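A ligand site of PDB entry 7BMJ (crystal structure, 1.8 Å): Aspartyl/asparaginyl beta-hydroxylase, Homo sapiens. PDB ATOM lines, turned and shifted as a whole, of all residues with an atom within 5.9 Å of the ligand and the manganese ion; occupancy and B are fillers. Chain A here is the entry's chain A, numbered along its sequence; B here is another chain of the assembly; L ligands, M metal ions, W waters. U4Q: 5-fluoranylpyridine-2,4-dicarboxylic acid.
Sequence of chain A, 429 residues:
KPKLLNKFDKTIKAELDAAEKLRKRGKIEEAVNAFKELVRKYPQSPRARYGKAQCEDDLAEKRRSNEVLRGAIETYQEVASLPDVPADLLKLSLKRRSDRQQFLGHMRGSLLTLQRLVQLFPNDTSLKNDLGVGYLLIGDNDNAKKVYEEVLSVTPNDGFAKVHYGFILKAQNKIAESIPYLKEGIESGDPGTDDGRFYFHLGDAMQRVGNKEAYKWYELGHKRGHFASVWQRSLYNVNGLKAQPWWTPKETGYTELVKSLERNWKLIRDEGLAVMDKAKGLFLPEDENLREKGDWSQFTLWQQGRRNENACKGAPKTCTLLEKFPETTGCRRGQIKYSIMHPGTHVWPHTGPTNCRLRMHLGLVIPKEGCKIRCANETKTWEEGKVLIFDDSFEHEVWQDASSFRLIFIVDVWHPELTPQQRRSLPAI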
ATOM      1  N   LEU A 290     -17.084 -23.407 -23.004  1.00  0.00           N
ATOM      2  CA  LEU A 290     -15.810 -22.854 -22.560  1.00  0.00           C
ATOM      3  C   LEU A 290     -15.844 -21.354 -22.309  1.00  0.00           C
ATOM      4  O   LEU A 290     -14.841 -20.793 -21.851  1.00  0.00           O
ATOM      5  CB  LEU A 290     -14.727 -23.185 -23.601  1.00  0.00           C
ATOM      6  CG  LEU A 290     -14.530 -24.676 -23.881  1.00  0.00           C
ATOM      7  CD1 LEU A 290     -13.693 -24.909 -25.136  1.00  0.00           C
ATOM      8  CD2 LEU A 290     -13.899 -25.387 -22.688  1.00  0.00           C
ATOM      9  N   TRP A 296     -17.843 -15.935 -29.434  1.00  0.00           N
ATOM     10  CA  TRP A 296     -16.700 -16.664 -29.995  1.00  0.00           C
ATOM     11  C   TRP A 296     -17.266 -17.671 -30.985  1.00  0.00           C
ATOM     12  O   TRP A 296     -18.106 -18.496 -30.599  1.00  0.00           O
ATOM     13  CB  TRP A 296     -15.911 -17.340 -28.877  1.00  0.00           C
ATOM     14  CG  TRP A 296     -14.788 -18.251 -29.300  1.00  0.00           C
ATOM     15  CD1 TRP A 296     -14.151 -18.270 -30.506  1.00  0.00           C
ATOM     16  CD2 TRP A 296     -14.189 -19.286 -28.510  1.00  0.00           C
ATOM     17  NE1 TRP A 296     -13.185 -19.257 -30.514  1.00  0.00           N
ATOM     18  CE2 TRP A 296     -13.182 -19.882 -29.293  1.00  0.00           C
ATOM     19  CE3 TRP A 296     -14.399 -19.747 -27.212  1.00  0.00           C
ATOM     20  CZ2 TRP A 296     -12.395 -20.931 -28.828  1.00  0.00           C
ATOM     21  CZ3 TRP A 296     -13.606 -20.789 -26.738  1.00  0.00           C
ATOM     22  CH2 TRP A 296     -12.619 -21.364 -27.552  1.00  0.00           C
ATOM     23  N   GLN A 298     -16.292 -20.053 -34.822  1.00  0.00           N
ATOM     24  CA  GLN A 298     -15.208 -20.689 -35.549  1.00  0.00           C
ATOM     25  C   GLN A 298     -15.703 -21.223 -36.884  1.00  0.00           C
ATOM     26  O   GLN A 298     -16.810 -21.748 -36.983  1.00  0.00           O
ATOM     27  CB  GLN A 298     -14.598 -21.816 -34.705  1.00  0.00           C
ATOM     28  CG  GLN A 298     -13.987 -21.288 -33.413  1.00  0.00           C
ATOM     29  CD  GLN A 298     -13.307 -22.363 -32.602  1.00  0.00           C
ATOM     30  OE1 GLN A 298     -12.192 -22.162 -32.095  1.00  0.00           O
ATOM     31  NE2 GLN A 298     -13.957 -23.514 -32.463  1.00  0.00           N
ATOM     32  N   LYS A 337      -8.919 -23.933 -38.629  1.00  0.00           N
ATOM     33  CA  LYS A 337     -10.111 -23.082 -38.591  1.00  0.00           C
ATOM     34  C   LYS A 337      -9.768 -21.628 -38.310  1.00  0.00           C
ATOM     35  O   LYS A 337      -8.759 -21.313 -37.673  1.00  0.00           O
ATOM     36  CB  LYS A 337     -11.090 -23.562 -37.516  1.00  0.00           C
ATOM     37  CG  LYS A 337     -10.518 -23.523 -36.122  1.00  0.00           C
ATOM     38  CD  LYS A 337     -11.269 -24.525 -35.242  1.00  0.00           C
ATOM     39  CE  LYS A 337     -10.942 -24.386 -33.770  1.00  0.00           C
ATOM     40  NZ  LYS A 337      -9.606 -24.907 -33.420  1.00  0.00           N
ATOM     41  N   SER A 339     -10.993 -18.316 -36.186  1.00  0.00           N
ATOM     42  CA  SER A 339     -11.651 -18.071 -34.910  1.00  0.00           C
ATOM     43  C   SER A 339     -11.818 -16.574 -34.732  1.00  0.00           C
ATOM     44  O   SER A 339     -10.823 -15.836 -34.727  1.00  0.00           O
ATOM     45  CB  SER A 339     -10.857 -18.677 -33.758  1.00  0.00           C
ATOM     46  OG  SER A 339     -11.416 -18.337 -32.507  1.00  0.00           O
ATOM     47  N   ILE A 340     -13.075 -16.119 -34.605  1.00  0.00           N
ATOM     48  CA  ILE A 340     -13.377 -14.729 -34.333  1.00  0.00           C
ATOM     49  C   ILE A 340     -13.912 -14.609 -32.905  1.00  0.00           C
ATOM     50  O   ILE A 340     -14.699 -15.447 -32.434  1.00  0.00           O
ATOM     51  CB  ILE A 340     -14.386 -14.142 -35.346  1.00  0.00           C
ATOM     52  CG1 ILE A 340     -14.716 -12.696 -34.981  1.00  0.00           C
ATOM     53  CG2 ILE A 340     -15.644 -14.956 -35.427  1.00  0.00           C
ATOM     54  CD1 ILE A 340     -15.056 -11.841 -36.176  1.00  0.00           C
ATOM     55  N   MET A 341     -13.440 -13.584 -32.215  1.00  0.00           N
ATOM     56  CA  MET A 341     -13.816 -13.303 -30.848  1.00  0.00           C
ATOM     57  C   MET A 341     -14.101 -11.804 -30.740  1.00  0.00           C
ATOM     58  O   MET A 341     -13.347 -10.992 -31.280  1.00  0.00           O
ATOM     59  CB  MET A 341     -12.707 -13.720 -29.878  1.00  0.00           C
ATOM     60  CG  MET A 341     -13.163 -13.756 -28.431  1.00  0.00           C
ATOM     61  SD  MET A 341     -11.928 -14.467 -27.336  1.00  0.00           S
ATOM     62  CE  MET A 341     -11.968 -16.192 -27.838  1.00  0.00           C
ATOM     63  N   VAL A 347     -12.702 -16.661 -21.949  1.00  0.00           N
ATOM     64  CA  VAL A 347     -12.733 -18.114 -22.082  1.00  0.00           C
ATOM     65  C   VAL A 347     -12.141 -18.720 -20.825  1.00  0.00           C
ATOM     66  O   VAL A 347     -11.026 -18.354 -20.417  1.00  0.00           O
ATOM     67  CB  VAL A 347     -11.972 -18.586 -23.342  1.00  0.00           C
ATOM     68  CG1 VAL A 347     -11.937 -20.109 -23.397  1.00  0.00           C
ATOM     69  CG2 VAL A 347     -12.639 -18.019 -24.584  1.00  0.00           C
ATOM     70  N   HIS A 350      -8.836 -23.932 -19.550  1.00  0.00           N
ATOM     71  CA  HIS A 350      -9.238 -25.238 -20.030  1.00  0.00           C
ATOM     72  C   HIS A 350      -8.048 -25.925 -20.682  1.00  0.00           C
ATOM     73  O   HIS A 350      -7.021 -25.298 -20.950  1.00  0.00           O
ATOM     74  CB  HIS A 350     -10.403 -25.150 -21.024  1.00  0.00           C
ATOM     75  CG  HIS A 350     -10.053 -24.432 -22.296  1.00  0.00           C
ATOM     76  ND1 HIS A 350      -9.875 -23.070 -22.363  1.00  0.00           N
ATOM     77  CD2 HIS A 350      -9.883 -24.901 -23.565  1.00  0.00           C
ATOM     78  CE1 HIS A 350      -9.578 -22.727 -23.603  1.00  0.00           C
ATOM     79  NE2 HIS A 350      -9.597 -23.809 -24.357  1.00  0.00           N
ATOM     80  N   GLY A 352      -7.049 -29.017 -23.765  1.00  0.00           N
ATOM     81  CA  GLY A 352      -7.455 -29.872 -24.852  1.00  0.00           C
ATOM     82  C   GLY A 352      -7.396 -31.343 -24.492  1.00  0.00           C
ATOM     83  O   GLY A 352      -6.855 -31.750 -23.449  1.00  0.00           O
ATOM     84  N   ARG A 357      -0.894 -33.069 -30.290  1.00  0.00           N
ATOM     85  CA  ARG A 357      -0.939 -31.960 -31.230  1.00  0.00           C
ATOM     86  C   ARG A 357      -0.333 -30.724 -30.589  1.00  0.00           C
ATOM     87  O   ARG A 357      -0.270 -30.596 -29.367  1.00  0.00           O
ATOM     88  CB  ARG A 357      -2.356 -31.648 -31.699  1.00  0.00           C
ATOM     89  CG  ARG A 357      -3.270 -31.157 -30.589  1.00  0.00           C
ATOM     90  CD  ARG A 357      -4.456 -30.430 -31.154  1.00  0.00           C
ATOM     91  NE  ARG A 357      -5.334 -29.873 -30.124  1.00  0.00           N
ATOM     92  CZ  ARG A 357      -6.623 -30.158 -29.997  1.00  0.00           C
ATOM     93  NH1 ARG A 357      -7.224 -30.993 -30.822  1.00  0.00           N
ATOM     94  NH2 ARG A 357      -7.326 -29.572 -29.031  1.00  0.00           N
ATOM     95  N   ARG A 359      -0.751 -26.349 -31.410  1.00  0.00           N
ATOM     96  CA  ARG A 359      -1.639 -25.402 -32.074  1.00  0.00           C
ATOM     97  C   ARG A 359      -0.847 -24.175 -32.520  1.00  0.00           C
ATOM     98  O   ARG A 359      -0.182 -23.541 -31.701  1.00  0.00           O
ATOM     99  CB  ARG A 359      -2.782 -24.968 -31.163  1.00  0.00           C
ATOM    100  CG  ARG A 359      -3.522 -26.099 -30.496  1.00  0.00           C
ATOM    101  CD  ARG A 359      -4.978 -25.702 -30.201  1.00  0.00           C
ATOM    102  NE  ARG A 359      -5.862 -26.270 -31.208  1.00  0.00           N
ATOM    103  CZ  ARG A 359      -7.178 -26.399 -31.069  1.00  0.00           C
ATOM    104  NH1 ARG A 359      -7.776 -25.963 -29.970  1.00  0.00           N
ATOM    105  NH2 ARG A 359      -7.875 -26.960 -32.037  1.00  0.00           N
ATOM    106  N   HIS A 361      -1.320 -20.382 -33.924  1.00  0.00           N
ATOM    107  CA  HIS A 361      -2.231 -19.245 -34.077  1.00  0.00           C
ATOM    108  C   HIS A 361      -1.566 -18.193 -34.951  1.00  0.00           C
ATOM    109  O   HIS A 361      -0.491 -17.693 -34.607  1.00  0.00           O
ATOM    110  CB  HIS A 361      -2.589 -18.620 -32.723  1.00  0.00           C
ATOM    111  CG  HIS A 361      -3.555 -19.407 -31.911  1.00  0.00           C
ATOM    112  ND1 HIS A 361      -4.142 -18.914 -30.759  1.00  0.00           N
ATOM    113  CD2 HIS A 361      -4.024 -20.678 -32.050  1.00  0.00           C
ATOM    114  CE1 HIS A 361      -4.923 -19.832 -30.230  1.00  0.00           C
ATOM    115  NE2 HIS A 361      -4.876 -20.914 -30.991  1.00  0.00           N
ATOM    116  N   ILE A 373      -3.698 -14.211 -24.445  1.00  0.00           N
ATOM    117  CA  ILE A 373      -3.819 -15.644 -24.229  1.00  0.00           C
ATOM    118  C   ILE A 373      -2.735 -16.064 -23.237  1.00  0.00           C
ATOM    119  O   ILE A 373      -1.553 -15.758 -23.445  1.00  0.00           O
ATOM    120  CB  ILE A 373      -3.716 -16.459 -25.531  1.00  0.00           C
ATOM    121  CG1 ILE A 373      -3.727 -17.956 -25.223  1.00  0.00           C
ATOM    122  CG2 ILE A 373      -2.456 -16.072 -26.306  1.00  0.00           C
ATOM    123  CD1 ILE A 373      -3.810 -18.861 -26.447  1.00  0.00           C
ATOM    124  N   TRP A 382      -1.303 -11.803 -29.600  1.00  0.00           N
ATOM    125  CA  TRP A 382      -1.170 -12.061 -31.019  1.00  0.00           C
ATOM    126  C   TRP A 382      -0.636 -10.825 -31.736  1.00  0.00           C
ATOM    127  O   TRP A 382      -0.706  -9.698 -31.224  1.00  0.00           O
ATOM    128  CB  TRP A 382      -2.503 -12.467 -31.638  1.00  0.00           C
ATOM    129  CG  TRP A 382      -3.084 -13.741 -31.076  1.00  0.00           C
ATOM    130  CD1 TRP A 382      -2.828 -15.001 -31.490  1.00  0.00           C
ATOM    131  CD2 TRP A 382      -4.043 -13.847 -30.007  1.00  0.00           C
ATOM    132  NE1 TRP A 382      -3.556 -15.907 -30.757  1.00  0.00           N
ATOM    133  CE2 TRP A 382      -4.308 -15.228 -29.827  1.00  0.00           C
ATOM    134  CE3 TRP A 382      -4.696 -12.919 -29.192  1.00  0.00           C
ATOM    135  CZ2 TRP A 382      -5.206 -15.707 -28.867  1.00  0.00           C
ATOM    136  CZ3 TRP A 382      -5.578 -13.394 -28.227  1.00  0.00           C
ATOM    137  CH2 TRP A 382      -5.822 -14.781 -28.069  1.00  0.00           C
ATOM    138  N   PHE A 390       1.589 -23.036 -29.219  1.00  0.00           N
ATOM    139  CA  PHE A 390       1.497 -23.541 -27.850  1.00  0.00           C
ATOM    140  C   PHE A 390       0.919 -24.952 -27.869  1.00  0.00           C
ATOM    141  O   PHE A 390       0.353 -25.418 -28.865  1.00  0.00           O
ATOM    142  CB  PHE A 390       0.643 -22.636 -26.936  1.00  0.00           C
ATOM    143  CG  PHE A 390      -0.806 -22.527 -27.346  1.00  0.00           C
ATOM    144  CD1 PHE A 390      -1.164 -21.808 -28.472  1.00  0.00           C
ATOM    145  CD2 PHE A 390      -1.801 -23.121 -26.591  1.00  0.00           C
ATOM    146  CE1 PHE A 390      -2.490 -21.701 -28.849  1.00  0.00           C
ATOM    147  CE2 PHE A 390      -3.140 -23.010 -26.950  1.00  0.00           C
ATOM    148  CZ  PHE A 390      -3.473 -22.288 -28.098  1.00  0.00           C
ATOM    149  N   ASP A 392      -1.859 -27.031 -26.370  1.00  0.00           N
ATOM    150  CA  ASP A 392      -3.123 -26.754 -25.706  1.00  0.00           C
ATOM    151  C   ASP A 392      -3.545 -27.873 -24.757  1.00  0.00           C
ATOM    152  O   ASP A 392      -4.627 -27.780 -24.172  1.00  0.00           O
ATOM    153  CB  ASP A 392      -4.223 -26.475 -26.733  1.00  0.00           C
ATOM    154  CG  ASP A 392      -4.887 -27.730 -27.250  1.00  0.00           C
ATOM    155  OD1 ASP A 392      -4.182 -28.705 -27.562  1.00  0.00           O
ATOM    156  OD2 ASP A 392      -6.131 -27.719 -27.371  1.00  0.00           O
ATOM    157  N   HIS A 396      -4.895 -23.319 -20.556  1.00  0.00           N
ATOM    158  CA  HIS A 396      -4.768 -22.030 -21.232  1.00  0.00           C
ATOM    159  C   HIS A 396      -6.089 -21.267 -21.098  1.00  0.00           C
ATOM    160  O   HIS A 396      -7.122 -21.844 -20.759  1.00  0.00           O
ATOM    161  CB  HIS A 396      -4.327 -22.189 -22.703  1.00  0.00           C
ATOM    162  CG  HIS A 396      -5.252 -23.018 -23.546  1.00  0.00           C
ATOM    163  ND1 HIS A 396      -5.298 -24.394 -23.465  1.00  0.00           N
ATOM    164  CD2 HIS A 396      -6.134 -22.669 -24.512  1.00  0.00           C
ATOM    165  CE1 HIS A 396      -6.195 -24.851 -24.318  1.00  0.00           C
ATOM    166  NE2 HIS A 396      -6.722 -23.827 -24.964  1.00  0.00           N
ATOM    167  N   VAL A 398      -8.124 -17.246 -22.307  1.00  0.00           N
ATOM    168  CA  VAL A 398      -8.135 -16.178 -23.292  1.00  0.00           C
ATOM    169  C   VAL A 398      -9.068 -15.069 -22.847  1.00  0.00           C
ATOM    170  O   VAL A 398     -10.118 -15.327 -22.241  1.00  0.00           O
ATOM    171  CB  VAL A 398      -8.532 -16.700 -24.693  1.00  0.00           C
ATOM    172  CG1 VAL A 398      -8.789 -15.548 -25.660  1.00  0.00           C
ATOM    173  CG2 VAL A 398      -7.458 -17.630 -25.220  1.00  0.00           C
ATOM    174  N   ARG A 406     -11.661  -9.554 -33.134  1.00  0.00           N
ATOM    175  CA  ARG A 406     -10.349 -10.167 -33.242  1.00  0.00           C
ATOM    176  C   ARG A 406     -10.471 -11.466 -34.018  1.00  0.00           C
ATOM    177  O   ARG A 406     -11.260 -12.352 -33.634  1.00  0.00           O
ATOM    178  CB  ARG A 406      -9.765 -10.450 -31.856  1.00  0.00           C
ATOM    179  CG  ARG A 406      -8.369 -11.096 -31.897  1.00  0.00           C
ATOM    180  CD  ARG A 406      -8.333 -12.326 -31.014  1.00  0.00           C
ATOM    181  NE  ARG A 406      -9.135 -13.404 -31.586  1.00  0.00           N
ATOM    182  CZ  ARG A 406      -9.241 -14.627 -31.063  1.00  0.00           C
ATOM    183  NH1 ARG A 406      -8.607 -14.943 -29.942  1.00  0.00           N
ATOM    184  NH2 ARG A 406      -9.975 -15.535 -31.674  1.00  0.00           N
ATOM    185  N   ILE A 408      -8.278 -14.731 -35.758  1.00  0.00           N
ATOM    186  CA  ILE A 408      -7.045 -15.505 -35.898  1.00  0.00           C
ATOM    187  C   ILE A 408      -7.325 -16.724 -36.752  1.00  0.00           C
ATOM    188  O   ILE A 408      -8.471 -17.088 -37.022  1.00  0.00           O
ATOM    189  CB  ILE A 408      -6.452 -15.927 -34.546  1.00  0.00           C
ATOM    190  CG1 ILE A 408      -7.374 -16.914 -33.821  1.00  0.00           C
ATOM    191  CG2 ILE A 408      -6.139 -14.707 -33.718  1.00  0.00           C
ATOM    192  CD1 ILE A 408      -6.820 -17.395 -32.486  1.00  0.00           C
ATOM    193  N   ILE A 410      -6.192 -20.810 -36.904  1.00  0.00           N
ATOM    194  CA  ILE A 410      -5.693 -21.861 -36.004  1.00  0.00           C
ATOM    195  C   ILE A 410      -5.358 -23.081 -36.827  1.00  0.00           C
ATOM    196  O   ILE A 410      -6.240 -23.649 -37.498  1.00  0.00           O
ATOM    197  CB  ILE A 410      -6.704 -22.204 -34.896  1.00  0.00           C
ATOM    198  CG1 ILE A 410      -7.093 -20.920 -34.124  1.00  0.00           C
ATOM    199  CG2 ILE A 410      -6.136 -23.260 -33.951  1.00  0.00           C
ATOM    200  CD1 ILE A 410      -8.129 -21.128 -33.031  1.00  0.00           C
ATOM    201  N   ASP A 412      -3.589 -26.779 -36.469  1.00  0.00           N
ATOM    202  CA  ASP A 412      -3.065 -27.827 -35.591  1.00  0.00           C
ATOM    203  C   ASP A 412      -2.065 -28.708 -36.332  1.00  0.00           C
ATOM    204  O   ASP A 412      -2.276 -29.075 -37.493  1.00  0.00           O
ATOM    205  CB  ASP A 412      -4.189 -28.713 -35.043  1.00  0.00           C
ATOM    206  CG  ASP A 412      -5.178 -27.937 -34.195  1.00  0.00           C
ATOM    207  OD1 ASP A 412      -4.756 -26.933 -33.566  1.00  0.00           O
ATOM    208  OD2 ASP A 412      -6.373 -28.334 -34.159  1.00  0.00           O
ATOM    209  N   ASP B  18     -11.741 -28.320 -28.535  1.00  0.00           N
ATOM    210  CA  ASP B  18     -10.923 -27.532 -27.629  1.00  0.00           C
ATOM    211  C   ASP B  18     -10.915 -28.075 -26.203  1.00  0.00           C
ATOM    212  O   ASP B  18     -10.062 -27.664 -25.406  1.00  0.00           O
ATOM    213  CB  ASP B  18     -11.400 -26.068 -27.597  1.00  0.00           C
ATOM    214  CG  ASP B  18     -10.434 -25.118 -28.306  1.00  0.00           C
ATOM    215  OD1 ASP B  18     -10.386 -25.156 -29.548  1.00  0.00           O
ATOM    216  OD2 ASP B  18      -9.730 -24.353 -27.622  1.00  0.00           O
HETATM  217  C10 U4Q L   1      -9.481 -19.796 -27.330  1.00  0.00           C
HETATM  218  C02 U4Q L   1      -7.132 -22.967 -28.874  1.00  0.00           C
HETATM  219  C04 U4Q L   1      -7.980 -21.820 -28.314  1.00  0.00           C
HETATM  220  C05 U4Q L   1      -8.184 -20.697 -29.098  1.00  0.00           C
HETATM  221  C06 U4Q L   1      -8.963 -19.665 -28.605  1.00  0.00           C
HETATM  222  C07 U4Q L   1      -9.192 -18.405 -29.427  1.00  0.00           C
HETATM  223  C12 U4Q L   1      -9.240 -20.949 -26.614  1.00  0.00           C
HETATM  224  F11 U4Q L   1     -10.256 -18.822 -26.774  1.00  0.00           F
HETATM  225  N13 U4Q L   1      -8.499 -21.926 -27.100  1.00  0.00           N
HETATM  226  O01 U4Q L   1      -6.564 -22.841 -29.983  1.00  0.00           O
HETATM  227  O03 U4Q L   1      -7.047 -24.051 -28.229  1.00  0.00           O
HETATM  228  O08 U4Q L   1      -8.795 -17.309 -28.945  1.00  0.00           O
HETATM  229  O09 U4Q L   1      -9.742 -18.466 -30.567  1.00  0.00           O
HETATM  230 MN    MN M   1      -8.241 -24.051 -26.334  1.00  0.00          MN
HETATM  231  O   HOH W   1      -8.148 -26.235 -26.290  1.00  0.00           O
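The guanidinium group of Arg 359 is in salt-bridge range of the side-chain carboxylate of Asp 392, at 3.5 Å. The backbone carbonyl oxygen of Asp 392 sits at hydrogen-bond distance from the backbone NH of Gly 352. The backbone carbonyl oxygen (O) of Ser 339 lies within hydrogen-bond range of the guanidinium group (NH2) of Arg 406. The backbone NH of Ile 410 lies within hydrogen-bond range of the backbone carbonyl oxygen of Lys 337, at 2.7 Å. The side-chain amino group (NZ) of Lys 337 is in salt-bridge range of the side-chain carboxylate (OD1) of Asp 18 of chain B (3.96 Å). OD1 of Asp 412 lies within salt-bridge range of NE of Arg 359 (2.7 Å). OE1 of Gln 298 sits at hydrogen-bond distance from NE1 of Trp 296 (3.5 Å). OG of Ser 339 lies within hydrogen-bond range of NE1 of Trp 296 (2.8 Å).
Water W1 bridges O of Asp 18 of chain B (2.5 Å) and OD2 of Asp 392 (2.7 Å).
O01 of the ligand lies within salt-bridge range of NH1 of Arg 359, 3.3 Å away. The guanidinium group (NH1) of Arg 406 lies within salt-bridge range of an oxygen (O08) of the ligand, 2.6 Å away. An oxygen (O09) of the ligand is in hydrogen-bond range of the side-chain hydroxyl (OG) of Ser 339. A ring nitrogen (NE2) of His 361 is in hydrogen-bond range of an oxygen (O01) of the ligand (2.8 Å).
Trp 296 touches the ligand. Met 341 touches the ligand (CE to F11, 3.3 Å). Val 347 touches the ligand (CG2 to F11, 3.3 Å). CZ2 of Trp 382 touches O08 of the ligand (3.9 Å). Phe 390 touches the ligand. OD2 of Asp 392 touches O03 of the ligand, 3.9 Å away. Val 398 touches the ligand (CG2 to F11, 3.4 Å). CD1 of Ile 408 touches O09 of the ligand (3.7 Å). Ile 410 touches the ligand. Hydrophobic or aromatic side chains that line the ligand: Trp 296, Met 341, Val 347, His 350, His 361, Trp 382, Phe 390, His 396, Val 398, Ile 408 and Ile 410. 16 residues have an atom within 4 Å of the ligand: Trp 296, Ser 339, Met 341, Val 347, His 350, Arg 359, His 361, Trp 382, Phe 390, Asp 392, His 396, Val 398, Arg 406, Ile 408, Ile 410 and Asp 18 of chain B. The nearest printed residue that does not touch the ligand is Gln 298 (4.7 Å).
The manganese ion is bound by the side-chain carboxylate (OD2) of Asp 18 of chain B (2.0 Å), a ring nitrogen (NE2) of His 396 (2.1 Å), water W1 (2.2 Å), an oxygen (O03) of the ligand (2.2 Å), a nitrogen (N13) of the ligand (2.3 Å) and a ring nitrogen (NE2) of His 350 (2.4 Å). The manganese ion has six donor atoms within binding distance.
The nearest printed residue that does not touch the manganese ion is Arg 359 (4.1 Å).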
